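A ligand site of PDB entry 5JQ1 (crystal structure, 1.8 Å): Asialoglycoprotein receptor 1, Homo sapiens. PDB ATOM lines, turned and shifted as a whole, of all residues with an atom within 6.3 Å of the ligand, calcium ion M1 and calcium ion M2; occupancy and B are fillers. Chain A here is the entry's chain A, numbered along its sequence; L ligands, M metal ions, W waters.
Calcium ion M2 is bound by the side-chain carboxylate of Asp 120, the side-chain carboxylate of Glu 107, an oxygen (O3) of the ligand, the side-chain amide oxygen of Asn 119, the side-chain amide oxygen of Gln 94, the side-chain carboxylate of Asp 96, the backbone carbonyl oxygen of Asp 120 and an oxygen (O2) of the ligand.
The backbone NH of Asp 97 lies within hydrogen-bond range of the side-chain carboxylate of Asp 120, at 2.7 Å.
OE2 of Glu 107 lies close to N of Trp 98, 3.2 Å away.
A ring nitrogen (NE2) of His 111 is in hydrogen-bond range of the side-chain amide nitrogen (ND2) of Asn 119.
OD1 of Asp 96 lies close to N of Trp 98, 3.4 Å away.
N of Asp 108 is in hydrogen-bond range of O of Asp 121 (3.2 Å).
OH of Tyr 127 sits at hydrogen-bond distance from OD2 of Asp 121 (2.7 Å).
N of Asp 121 lies within hydrogen-bond range of O of Cys 109 (2.8 Å).
The side-chain amide nitrogen of Asn 63 lies close to a ring nitrogen (ND1) of His 111 (3.3 Å).
Water W5 lies within hydrogen-bond range of OD2 of Asp 121 (2.7 Å) and N1 of the ligand (3.1 Å).
Of the 23 residues printed, 4 come within 4 Å of calcium ion M1.
The nearest printed residue that does not touch calcium ion M1 is Asp 120 (4.6 Å).
Calcium ion M1 is bound by water W3 (2.4 Å), the side-chain carboxylate (OD1) of Asp 97 (2.4 Å), the backbone carbonyl oxygen (O) of Glu 107 (2.5 Å), the side-chain carboxylate (OD2) of Asp 70 (2.5 Å), the side-chain carboxylate (OD1) of Asp 108 (2.6 Å), water W1 (2.6 Å) and the side-chain carboxylate (OD1) of Asp 70 (2.7 Å).
Calcium ion M1 has seven donor atoms within binding distance.
Residues that only touch the ligand: Trp 98 (3.8 Å), His 111 (3.96 Å), Asp 121 (3.8 Å) and Tyr 127 (3.9 Å).
Hydrophobic or aromatic side chains within 4 Å of the ligand: Trp 98 and His 111.
Nine residues have an atom within 4 Å of the ligand: Gln 94, Asp 96, Trp 98, Glu 107, His 111, Asn 119, Asp 120, Asp 121 and Tyr 127.
The nearest printed residue that does not touch the ligand is Thr 113 (4.2 Å).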
ATOM      1  N   ASN A  63      -1.496  25.088  -8.153  1.00  0.00           N
ATOM      2  CA  ASN A  63      -2.688  24.565  -8.861  1.00  0.00           C
ATOM      3  C   ASN A  63      -3.840  25.486  -8.593  1.00  0.00           C
ATOM      4  O   ASN A  63      -4.110  25.790  -7.432  1.00  0.00           O
ATOM      5  CB  ASN A  63      -3.024  23.138  -8.456  1.00  0.00           C
ATOM      6  CG  ASN A  63      -1.983  22.123  -8.858  1.00  0.00           C
ATOM      7  OD1 ASN A  63      -1.650  21.194  -8.121  1.00  0.00           O
ATOM      8  ND2 ASN A  63      -1.536  22.212 -10.065  1.00  0.00           N
ATOM      9  N   ASP A  70     -15.526  20.175 -18.866  1.00  0.00           N
ATOM     10  CA  ASP A  70     -16.256  19.343 -19.828  1.00  0.00           C
ATOM     11  C   ASP A  70     -17.294  18.496 -19.085  1.00  0.00           C
ATOM     12  O   ASP A  70     -17.613  17.376 -19.499  1.00  0.00           O
ATOM     13  CB  ASP A  70     -15.282  18.454 -20.668  1.00  0.00           C
ATOM     14  CG  ASP A  70     -14.670  17.273 -19.944  1.00  0.00           C
ATOM     15  OD1 ASP A  70     -14.584  17.313 -18.697  1.00  0.00           O
ATOM     16  OD2 ASP A  70     -14.252  16.311 -20.621  1.00  0.00           O
ATOM     17  N   GLN A  71     -17.867  19.073 -18.014  1.00  0.00           N
ATOM     18  CA  GLN A  71     -18.893  18.395 -17.214  1.00  0.00           C
ATOM     19  C   GLN A  71     -20.155  18.025 -18.000  1.00  0.00           C
ATOM     20  O   GLN A  71     -20.800  17.053 -17.636  1.00  0.00           O
ATOM     21  CB  GLN A  71     -19.280  19.200 -15.959  1.00  0.00           C
ATOM     22  CG  GLN A  71     -18.111  19.486 -15.040  1.00  0.00           C
ATOM     23  CD  GLN A  71     -18.562  20.240 -13.833  1.00  0.00           C
ATOM     24  OE1 GLN A  71     -18.558  21.466 -13.808  1.00  0.00           O
ATOM     25  NE2 GLN A  71     -18.919  19.513 -12.790  1.00  0.00           N
ATOM     26  N   GLY A  73     -20.200  17.537 -21.436  1.00  0.00           N
ATOM     27  CA  GLY A  73     -19.801  16.899 -22.685  1.00  0.00           C
ATOM     28  C   GLY A  73     -18.538  17.498 -23.221  1.00  0.00           C
ATOM     29  O   GLY A  73     -17.445  17.079 -22.833  1.00  0.00           O
ATOM     30  N   TRP A  75     -15.560  20.401 -24.026  1.00  0.00           N
ATOM     31  CA  TRP A  75     -14.889  21.492 -23.301  1.00  0.00           C
ATOM     32  C   TRP A  75     -15.658  22.819 -23.526  1.00  0.00           C
ATOM     33  O   TRP A  75     -16.018  23.140 -24.657  1.00  0.00           O
ATOM     34  CB  TRP A  75     -13.424  21.646 -23.762  1.00  0.00           C
ATOM     35  CG  TRP A  75     -12.564  20.554 -23.186  1.00  0.00           C
ATOM     36  CD1 TRP A  75     -12.104  19.444 -23.833  1.00  0.00           C
ATOM     37  CD2 TRP A  75     -12.237  20.377 -21.804  1.00  0.00           C
ATOM     38  NE1 TRP A  75     -11.421  18.636 -22.949  1.00  0.00           N
ATOM     39  CE2 TRP A  75     -11.523  19.160 -21.693  1.00  0.00           C
ATOM     40  CE3 TRP A  75     -12.441  21.150 -20.647  1.00  0.00           C
ATOM     41  CZ2 TRP A  75     -11.047  18.684 -20.452  1.00  0.00           C
ATOM     42  CZ3 TRP A  75     -11.978  20.673 -19.424  1.00  0.00           C
ATOM     43  CH2 TRP A  75     -11.306  19.436 -19.341  1.00  0.00           C
ATOM     44  N   ARG A  91      -0.884  21.116 -20.585  1.00  0.00           N
ATOM     45  CA  ARG A  91       0.393  20.483 -20.270  1.00  0.00           C
ATOM     46  C   ARG A  91       0.548  19.271 -21.244  1.00  0.00           C
ATOM     47  O   ARG A  91      -0.472  18.727 -21.717  1.00  0.00           O
ATOM     48  CB  ARG A  91       0.386  20.000 -18.792  1.00  0.00           C
ATOM     49  CG  ARG A  91       1.605  20.509 -18.034  1.00  0.00           C
ATOM     50  CD  ARG A  91       1.690  19.928 -16.662  1.00  0.00           C
ATOM     51  NE  ARG A  91       3.063  19.592 -16.293  1.00  0.00           N
ATOM     52  CZ  ARG A  91       3.730  20.152 -15.294  1.00  0.00           C
ATOM     53  NH1 ARG A  91       3.153  21.110 -14.559  1.00  0.00           N
ATOM     54  NH2 ARG A  91       4.961  19.773 -15.009  1.00  0.00           N
ATOM     55  N   GLU A  93       0.470  15.594 -22.685  1.00  0.00           N
ATOM     56  CA  GLU A  93      -0.320  14.413 -22.309  1.00  0.00           C
ATOM     57  C   GLU A  93      -1.635  14.804 -21.605  1.00  0.00           C
ATOM     58  O   GLU A  93      -2.321  13.932 -21.084  1.00  0.00           O
ATOM     59  CB  GLU A  93       0.471  13.387 -21.449  1.00  0.00           C
ATOM     60  CG  GLU A  93       1.730  12.830 -22.107  1.00  0.00           C
ATOM     61  CD  GLU A  93       2.352  11.684 -21.320  1.00  0.00           C
ATOM     62  OE1 GLU A  93       2.257  10.536 -21.789  1.00  0.00           O
ATOM     63  OE2 GLU A  93       2.867  11.938 -20.203  1.00  0.00           O
ATOM     64  N   GLN A  94      -1.982  16.100 -21.597  1.00  0.00           N
ATOM     65  CA  GLN A  94      -3.273  16.530 -21.052  1.00  0.00           C
ATOM     66  C   GLN A  94      -4.128  17.133 -22.189  1.00  0.00           C
ATOM     67  O   GLN A  94      -3.563  17.644 -23.163  1.00  0.00           O
ATOM     68  CB  GLN A  94      -3.109  17.552 -19.894  1.00  0.00           C
ATOM     69  CG  GLN A  94      -2.259  17.065 -18.716  1.00  0.00           C
ATOM     70  CD  GLN A  94      -2.744  15.783 -18.065  1.00  0.00           C
ATOM     71  OE1 GLN A  94      -3.959  15.434 -18.093  1.00  0.00           O
ATOM     72  NE2 GLN A  94      -1.806  15.150 -17.359  1.00  0.00           N
ATOM     73  N   PRO A  95      -5.464  17.177 -22.048  1.00  0.00           N
ATOM     74  CA  PRO A  95      -6.274  16.576 -20.968  1.00  0.00           C
ATOM     75  C   PRO A  95      -6.343  15.057 -21.171  1.00  0.00           C
ATOM     76  O   PRO A  95      -6.231  14.570 -22.312  1.00  0.00           O
ATOM     77  CB  PRO A  95      -7.630  17.278 -21.122  1.00  0.00           C
ATOM     78  CG  PRO A  95      -7.729  17.635 -22.603  1.00  0.00           C
ATOM     79  CD  PRO A  95      -6.311  17.763 -23.121  1.00  0.00           C
ATOM     80  N   ASP A  96      -6.517  14.295 -20.111  1.00  0.00           N
ATOM     81  CA  ASP A  96      -6.541  12.840 -20.273  1.00  0.00           C
ATOM     82  C   ASP A  96      -7.745  12.143 -19.617  1.00  0.00           C
ATOM     83  O   ASP A  96      -7.833  10.904 -19.683  1.00  0.00           O
ATOM     84  CB  ASP A  96      -5.212  12.249 -19.781  1.00  0.00           C
ATOM     85  CG  ASP A  96      -5.007  12.446 -18.268  1.00  0.00           C
ATOM     86  OD1 ASP A  96      -5.835  13.155 -17.645  1.00  0.00           O
ATOM     87  OD2 ASP A  96      -4.029  11.928 -17.740  1.00  0.00           O
ATOM     88  N   ASP A  97      -8.637  12.906 -18.959  1.00  0.00           N
ATOM     89  CA  ASP A  97      -9.833  12.375 -18.264  1.00  0.00           C
ATOM     90  C   ASP A  97      -9.497  11.154 -17.386  1.00  0.00           C
ATOM     91  O   ASP A  97     -10.122  10.101 -17.502  1.00  0.00           O
ATOM     92  CB  ASP A  97     -10.893  11.991 -19.314  1.00  0.00           C
ATOM     93  CG  ASP A  97     -12.313  11.845 -18.781  1.00  0.00           C
ATOM     94  OD1 ASP A  97     -12.747  12.689 -17.962  1.00  0.00           O
ATOM     95  OD2 ASP A  97     -12.988  10.871 -19.173  1.00  0.00           O
ATOM     96  N   TRP A  98      -8.423  11.255 -16.618  1.00  0.00           N
ATOM     97  CA  TRP A  98      -7.913  10.141 -15.801  1.00  0.00           C
ATOM     98  C   TRP A  98      -8.960   9.638 -14.780  1.00  0.00           C
ATOM     99  O   TRP A  98      -9.547  10.446 -14.065  1.00  0.00           O
ATOM    100  CB  TRP A  98      -6.614  10.589 -15.091  1.00  0.00           C
ATOM    101  CG  TRP A  98      -5.861   9.505 -14.367  1.00  0.00           C
ATOM    102  CD1 TRP A  98      -5.419   8.317 -14.879  1.00  0.00           C
ATOM    103  CD2 TRP A  98      -5.335   9.602 -13.023  1.00  0.00           C
ATOM    104  NE1 TRP A  98      -4.687   7.643 -13.918  1.00  0.00           N
ATOM    105  CE2 TRP A  98      -4.626   8.398 -12.777  1.00  0.00           C
ATOM    106  CE3 TRP A  98      -5.431  10.561 -12.001  1.00  0.00           C
ATOM    107  CZ2 TRP A  98      -3.975   8.165 -11.552  1.00  0.00           C
ATOM    108  CZ3 TRP A  98      -4.806  10.320 -10.790  1.00  0.00           C
ATOM    109  CH2 TRP A  98      -4.122   9.107 -10.557  1.00  0.00           C
ATOM    110  N   GLY A 106     -14.107  10.577 -14.331  1.00  0.00           N
ATOM    111  CA  GLY A 106     -12.827  10.931 -14.946  1.00  0.00           C
ATOM    112  C   GLY A 106     -12.303  12.233 -14.345  1.00  0.00           C
ATOM    113  O   GLY A 106     -12.142  12.336 -13.117  1.00  0.00           O
ATOM    114  N   GLU A 107     -12.003  13.212 -15.185  1.00  0.00           N
ATOM    115  CA  GLU A 107     -11.490  14.531 -14.731  1.00  0.00           C
ATOM    116  C   GLU A 107     -12.132  15.550 -15.624  1.00  0.00           C
ATOM    117  O   GLU A 107     -11.961  15.464 -16.837  1.00  0.00           O
ATOM    118  CB  GLU A 107      -9.972  14.593 -14.882  1.00  0.00           C
ATOM    119  CG  GLU A 107      -9.254  13.877 -13.764  1.00  0.00           C
ATOM    120  CD  GLU A 107      -7.770  13.798 -13.963  1.00  0.00           C
ATOM    121  OE1 GLU A 107      -7.057  13.660 -12.939  1.00  0.00           O
ATOM    122  OE2 GLU A 107      -7.309  13.873 -15.130  1.00  0.00           O
ATOM    123  N   ASP A 108     -12.935  16.473 -15.049  1.00  0.00           N
ATOM    124  CA  ASP A 108     -13.735  17.361 -15.880  1.00  0.00           C
ATOM    125  C   ASP A 108     -13.483  18.866 -15.748  1.00  0.00           C
ATOM    126  O   ASP A 108     -14.193  19.621 -16.406  1.00  0.00           O
ATOM    127  CB  ASP A 108     -15.238  17.065 -15.601  1.00  0.00           C
ATOM    128  CG  ASP A 108     -15.680  15.640 -15.915  1.00  0.00           C
ATOM    129  OD1 ASP A 108     -14.905  14.904 -16.562  1.00  0.00           O
ATOM    130  OD2 ASP A 108     -16.838  15.310 -15.646  1.00  0.00           O
ATOM    131  N   CYS A 109     -12.553  19.301 -14.857  1.00  0.00           N
ATOM    132  CA  CYS A 109     -12.318  20.713 -14.567  1.00  0.00           C
ATOM    133  C   CYS A 109     -10.873  21.114 -14.853  1.00  0.00           C
ATOM    134  O   CYS A 109      -9.953  20.419 -14.454  1.00  0.00           O
ATOM    135  CB  CYS A 109     -12.733  21.033 -13.124  1.00  0.00           C
ATOM    136  SG  CYS A 109     -14.527  20.990 -12.840  1.00  0.00           S
ATOM    137  N   HIS A 111      -7.403  23.375 -14.566  1.00  0.00           N
ATOM    138  CA  HIS A 111      -6.650  24.219 -13.664  1.00  0.00           C
ATOM    139  C   HIS A 111      -5.264  24.516 -14.250  1.00  0.00           C
ATOM    140  O   HIS A 111      -4.733  23.728 -15.019  1.00  0.00           O
ATOM    141  CB  HIS A 111      -6.527  23.580 -12.236  1.00  0.00           C
ATOM    142  CG  HIS A 111      -5.667  22.345 -12.155  1.00  0.00           C
ATOM    143  ND1 HIS A 111      -4.324  22.418 -11.777  1.00  0.00           N
ATOM    144  CD2 HIS A 111      -5.989  21.049 -12.396  1.00  0.00           C
ATOM    145  CE1 HIS A 111      -3.893  21.166 -11.792  1.00  0.00           C
ATOM    146  NE2 HIS A 111      -4.831  20.318 -12.191  1.00  0.00           N
ATOM    147  N   THR A 113      -1.405  24.428 -13.812  1.00  0.00           N
ATOM    148  CA  THR A 113      -0.490  23.628 -12.993  1.00  0.00           C
ATOM    149  C   THR A 113       0.649  24.534 -12.485  1.00  0.00           C
ATOM    150  O   THR A 113       0.666  25.742 -12.773  1.00  0.00           O
ATOM    151  CB  THR A 113       0.094  22.439 -13.767  1.00  0.00           C
ATOM    152  OG1 THR A 113       0.872  22.953 -14.843  1.00  0.00           O
ATOM    153  CG2 THR A 113      -0.975  21.470 -14.258  1.00  0.00           C
ATOM    154  N   ASN A 119      -4.155  21.371 -16.854  1.00  0.00           N
ATOM    155  CA  ASN A 119      -4.477  19.988 -16.555  1.00  0.00           C
ATOM    156  C   ASN A 119      -5.966  19.876 -16.285  1.00  0.00           C
ATOM    157  O   ASN A 119      -6.545  20.804 -15.753  1.00  0.00           O
ATOM    158  CB  ASN A 119      -3.694  19.496 -15.330  1.00  0.00           C
ATOM    159  CG  ASN A 119      -4.036  18.070 -14.965  1.00  0.00           C
ATOM    160  OD1 ASN A 119      -4.129  17.202 -15.826  1.00  0.00           O
ATOM    161  ND2 ASN A 119      -4.466  17.867 -13.739  1.00  0.00           N
ATOM    162  N   ASP A 120      -6.582  18.733 -16.626  1.00  0.00           N
ATOM    163  CA  ASP A 120      -7.978  18.467 -16.262  1.00  0.00           C
ATOM    164  C   ASP A 120      -7.888  17.634 -14.966  1.00  0.00           C
ATOM    165  O   ASP A 120      -7.048  16.747 -14.856  1.00  0.00           O
ATOM    166  CB  ASP A 120      -8.738  17.693 -17.355  1.00  0.00           C
ATOM    167  CG  ASP A 120      -8.149  16.366 -17.788  1.00  0.00           C
ATOM    168  OD1 ASP A 120      -6.884  16.219 -17.767  1.00  0.00           O
ATOM    169  OD2 ASP A 120      -8.919  15.541 -18.335  1.00  0.00           O
ATOM    170  N   ASP A 121      -8.691  17.970 -13.961  1.00  0.00           N
ATOM    171  CA  ASP A 121      -8.664  17.264 -12.676  1.00  0.00           C
ATOM    172  C   ASP A 121     -10.079  17.070 -12.166  1.00  0.00           C
ATOM    173  O   ASP A 121     -11.052  17.554 -12.740  1.00  0.00           O
ATOM    174  CB  ASP A 121      -7.793  18.055 -11.633  1.00  0.00           C
ATOM    175  CG  ASP A 121      -7.064  17.181 -10.632  1.00  0.00           C
ATOM    176  OD1 ASP A 121      -7.535  16.054 -10.361  1.00  0.00           O
ATOM    177  OD2 ASP A 121      -5.941  17.578 -10.196  1.00  0.00           O
ATOM    178  N   VAL A 122     -10.177  16.359 -11.049  1.00  0.00           N
ATOM    179  CA  VAL A 122     -11.414  16.043 -10.368  1.00  0.00           C
ATOM    180  C   VAL A 122     -11.982  17.355  -9.852  1.00  0.00           C
ATOM    181  O   VAL A 122     -11.327  18.054  -9.065  1.00  0.00           O
ATOM    182  CB  VAL A 122     -11.077  15.030  -9.249  1.00  0.00           C
ATOM    183  CG1 VAL A 122     -12.296  14.710  -8.403  1.00  0.00           C
ATOM    184  CG2 VAL A 122     -10.495  13.748  -9.847  1.00  0.00           C
ATOM    185  N   TYR A 127      -8.783  23.753  -4.801  1.00  0.00           N
ATOM    186  CA  TYR A 127      -7.651  24.487  -5.323  1.00  0.00           C
ATOM    187  C   TYR A 127      -7.991  25.944  -5.213  1.00  0.00           C
ATOM    188  O   TYR A 127      -9.179  26.321  -5.131  1.00  0.00           O
ATOM    189  CB  TYR A 127      -7.422  24.187  -6.842  1.00  0.00           C
ATOM    190  CG  TYR A 127      -6.801  22.867  -7.222  1.00  0.00           C
ATOM    191  CD1 TYR A 127      -5.826  22.272  -6.417  1.00  0.00           C
ATOM    192  CD2 TYR A 127      -7.076  22.282  -8.453  1.00  0.00           C
ATOM    193  CE1 TYR A 127      -5.214  21.064  -6.775  1.00  0.00           C
ATOM    194  CE2 TYR A 127      -6.500  21.068  -8.823  1.00  0.00           C
ATOM    195  CZ  TYR A 127      -5.551  20.475  -7.991  1.00  0.00           C
ATOM    196  OH  TYR A 127      -4.927  19.329  -8.427  1.00  0.00           O
HETATM  197  C1  LIG L   1      -3.746  14.151 -13.348  1.00  0.00           C
HETATM  198  C2  LIG L   1      -1.854  11.998 -12.567  1.00  0.00           C
HETATM  199  C3  LIG L   1      -2.144  12.299 -14.097  1.00  0.00           C
HETATM  200  C4  LIG L   1      -1.954  11.101 -15.071  1.00  0.00           C
HETATM  201  C5  LIG L   1      -1.161  14.131 -13.216  1.00  0.00           C
HETATM  202  O1  LIG L   1      -1.338  17.528 -12.862  1.00  0.00           O
HETATM  203  C6  LIG L   1      -1.967  17.091 -11.941  1.00  0.00           C
HETATM  204  C7  LIG L   1      -2.142  17.816 -10.614  1.00  0.00           C
HETATM  205  N1  LIG L   1      -2.559  15.841 -12.056  1.00  0.00           N
HETATM  206  C8  LIG L   1      -2.471  15.018 -13.260  1.00  0.00           C
HETATM  207  O2  LIG L   1      -4.838  14.960 -13.646  1.00  0.00           O
HETATM  208  C9  LIG L   1      -3.556  12.960 -14.334  1.00  0.00           C
HETATM  209  O3  LIG L   1      -3.668  13.546 -15.628  1.00  0.00           O
HETATM  210  O4  LIG L   1      -0.642  10.672 -15.088  1.00  0.00           O
HETATM  211  O5  LIG L   1      -1.172  13.298 -14.374  1.00  0.00           O
HETATM  212  O6  LIG L   1      -1.202  13.212 -12.123  1.00  0.00           O
HETATM  213 CA    CA M   1     -13.498  14.894 -18.702  1.00  0.00          CA
HETATM  214 CA    CA M   2      -5.495  15.145 -16.125  1.00  0.00          CA
HETATM  215  O   HOH W   1     -13.414  13.661 -21.046  1.00  0.00           O
HETATM  216  O   HOH W   2       1.023  19.069 -12.229  1.00  0.00           O
HETATM  217  O   HOH W   3     -11.319  15.378 -19.633  1.00  0.00           O
HETATM  218  O   HOH W   4      -0.349  17.694 -15.370  1.00  0.00           O
HETATM  219  O   HOH W   5      -4.530  15.312  -9.773  1.00  0.00           O
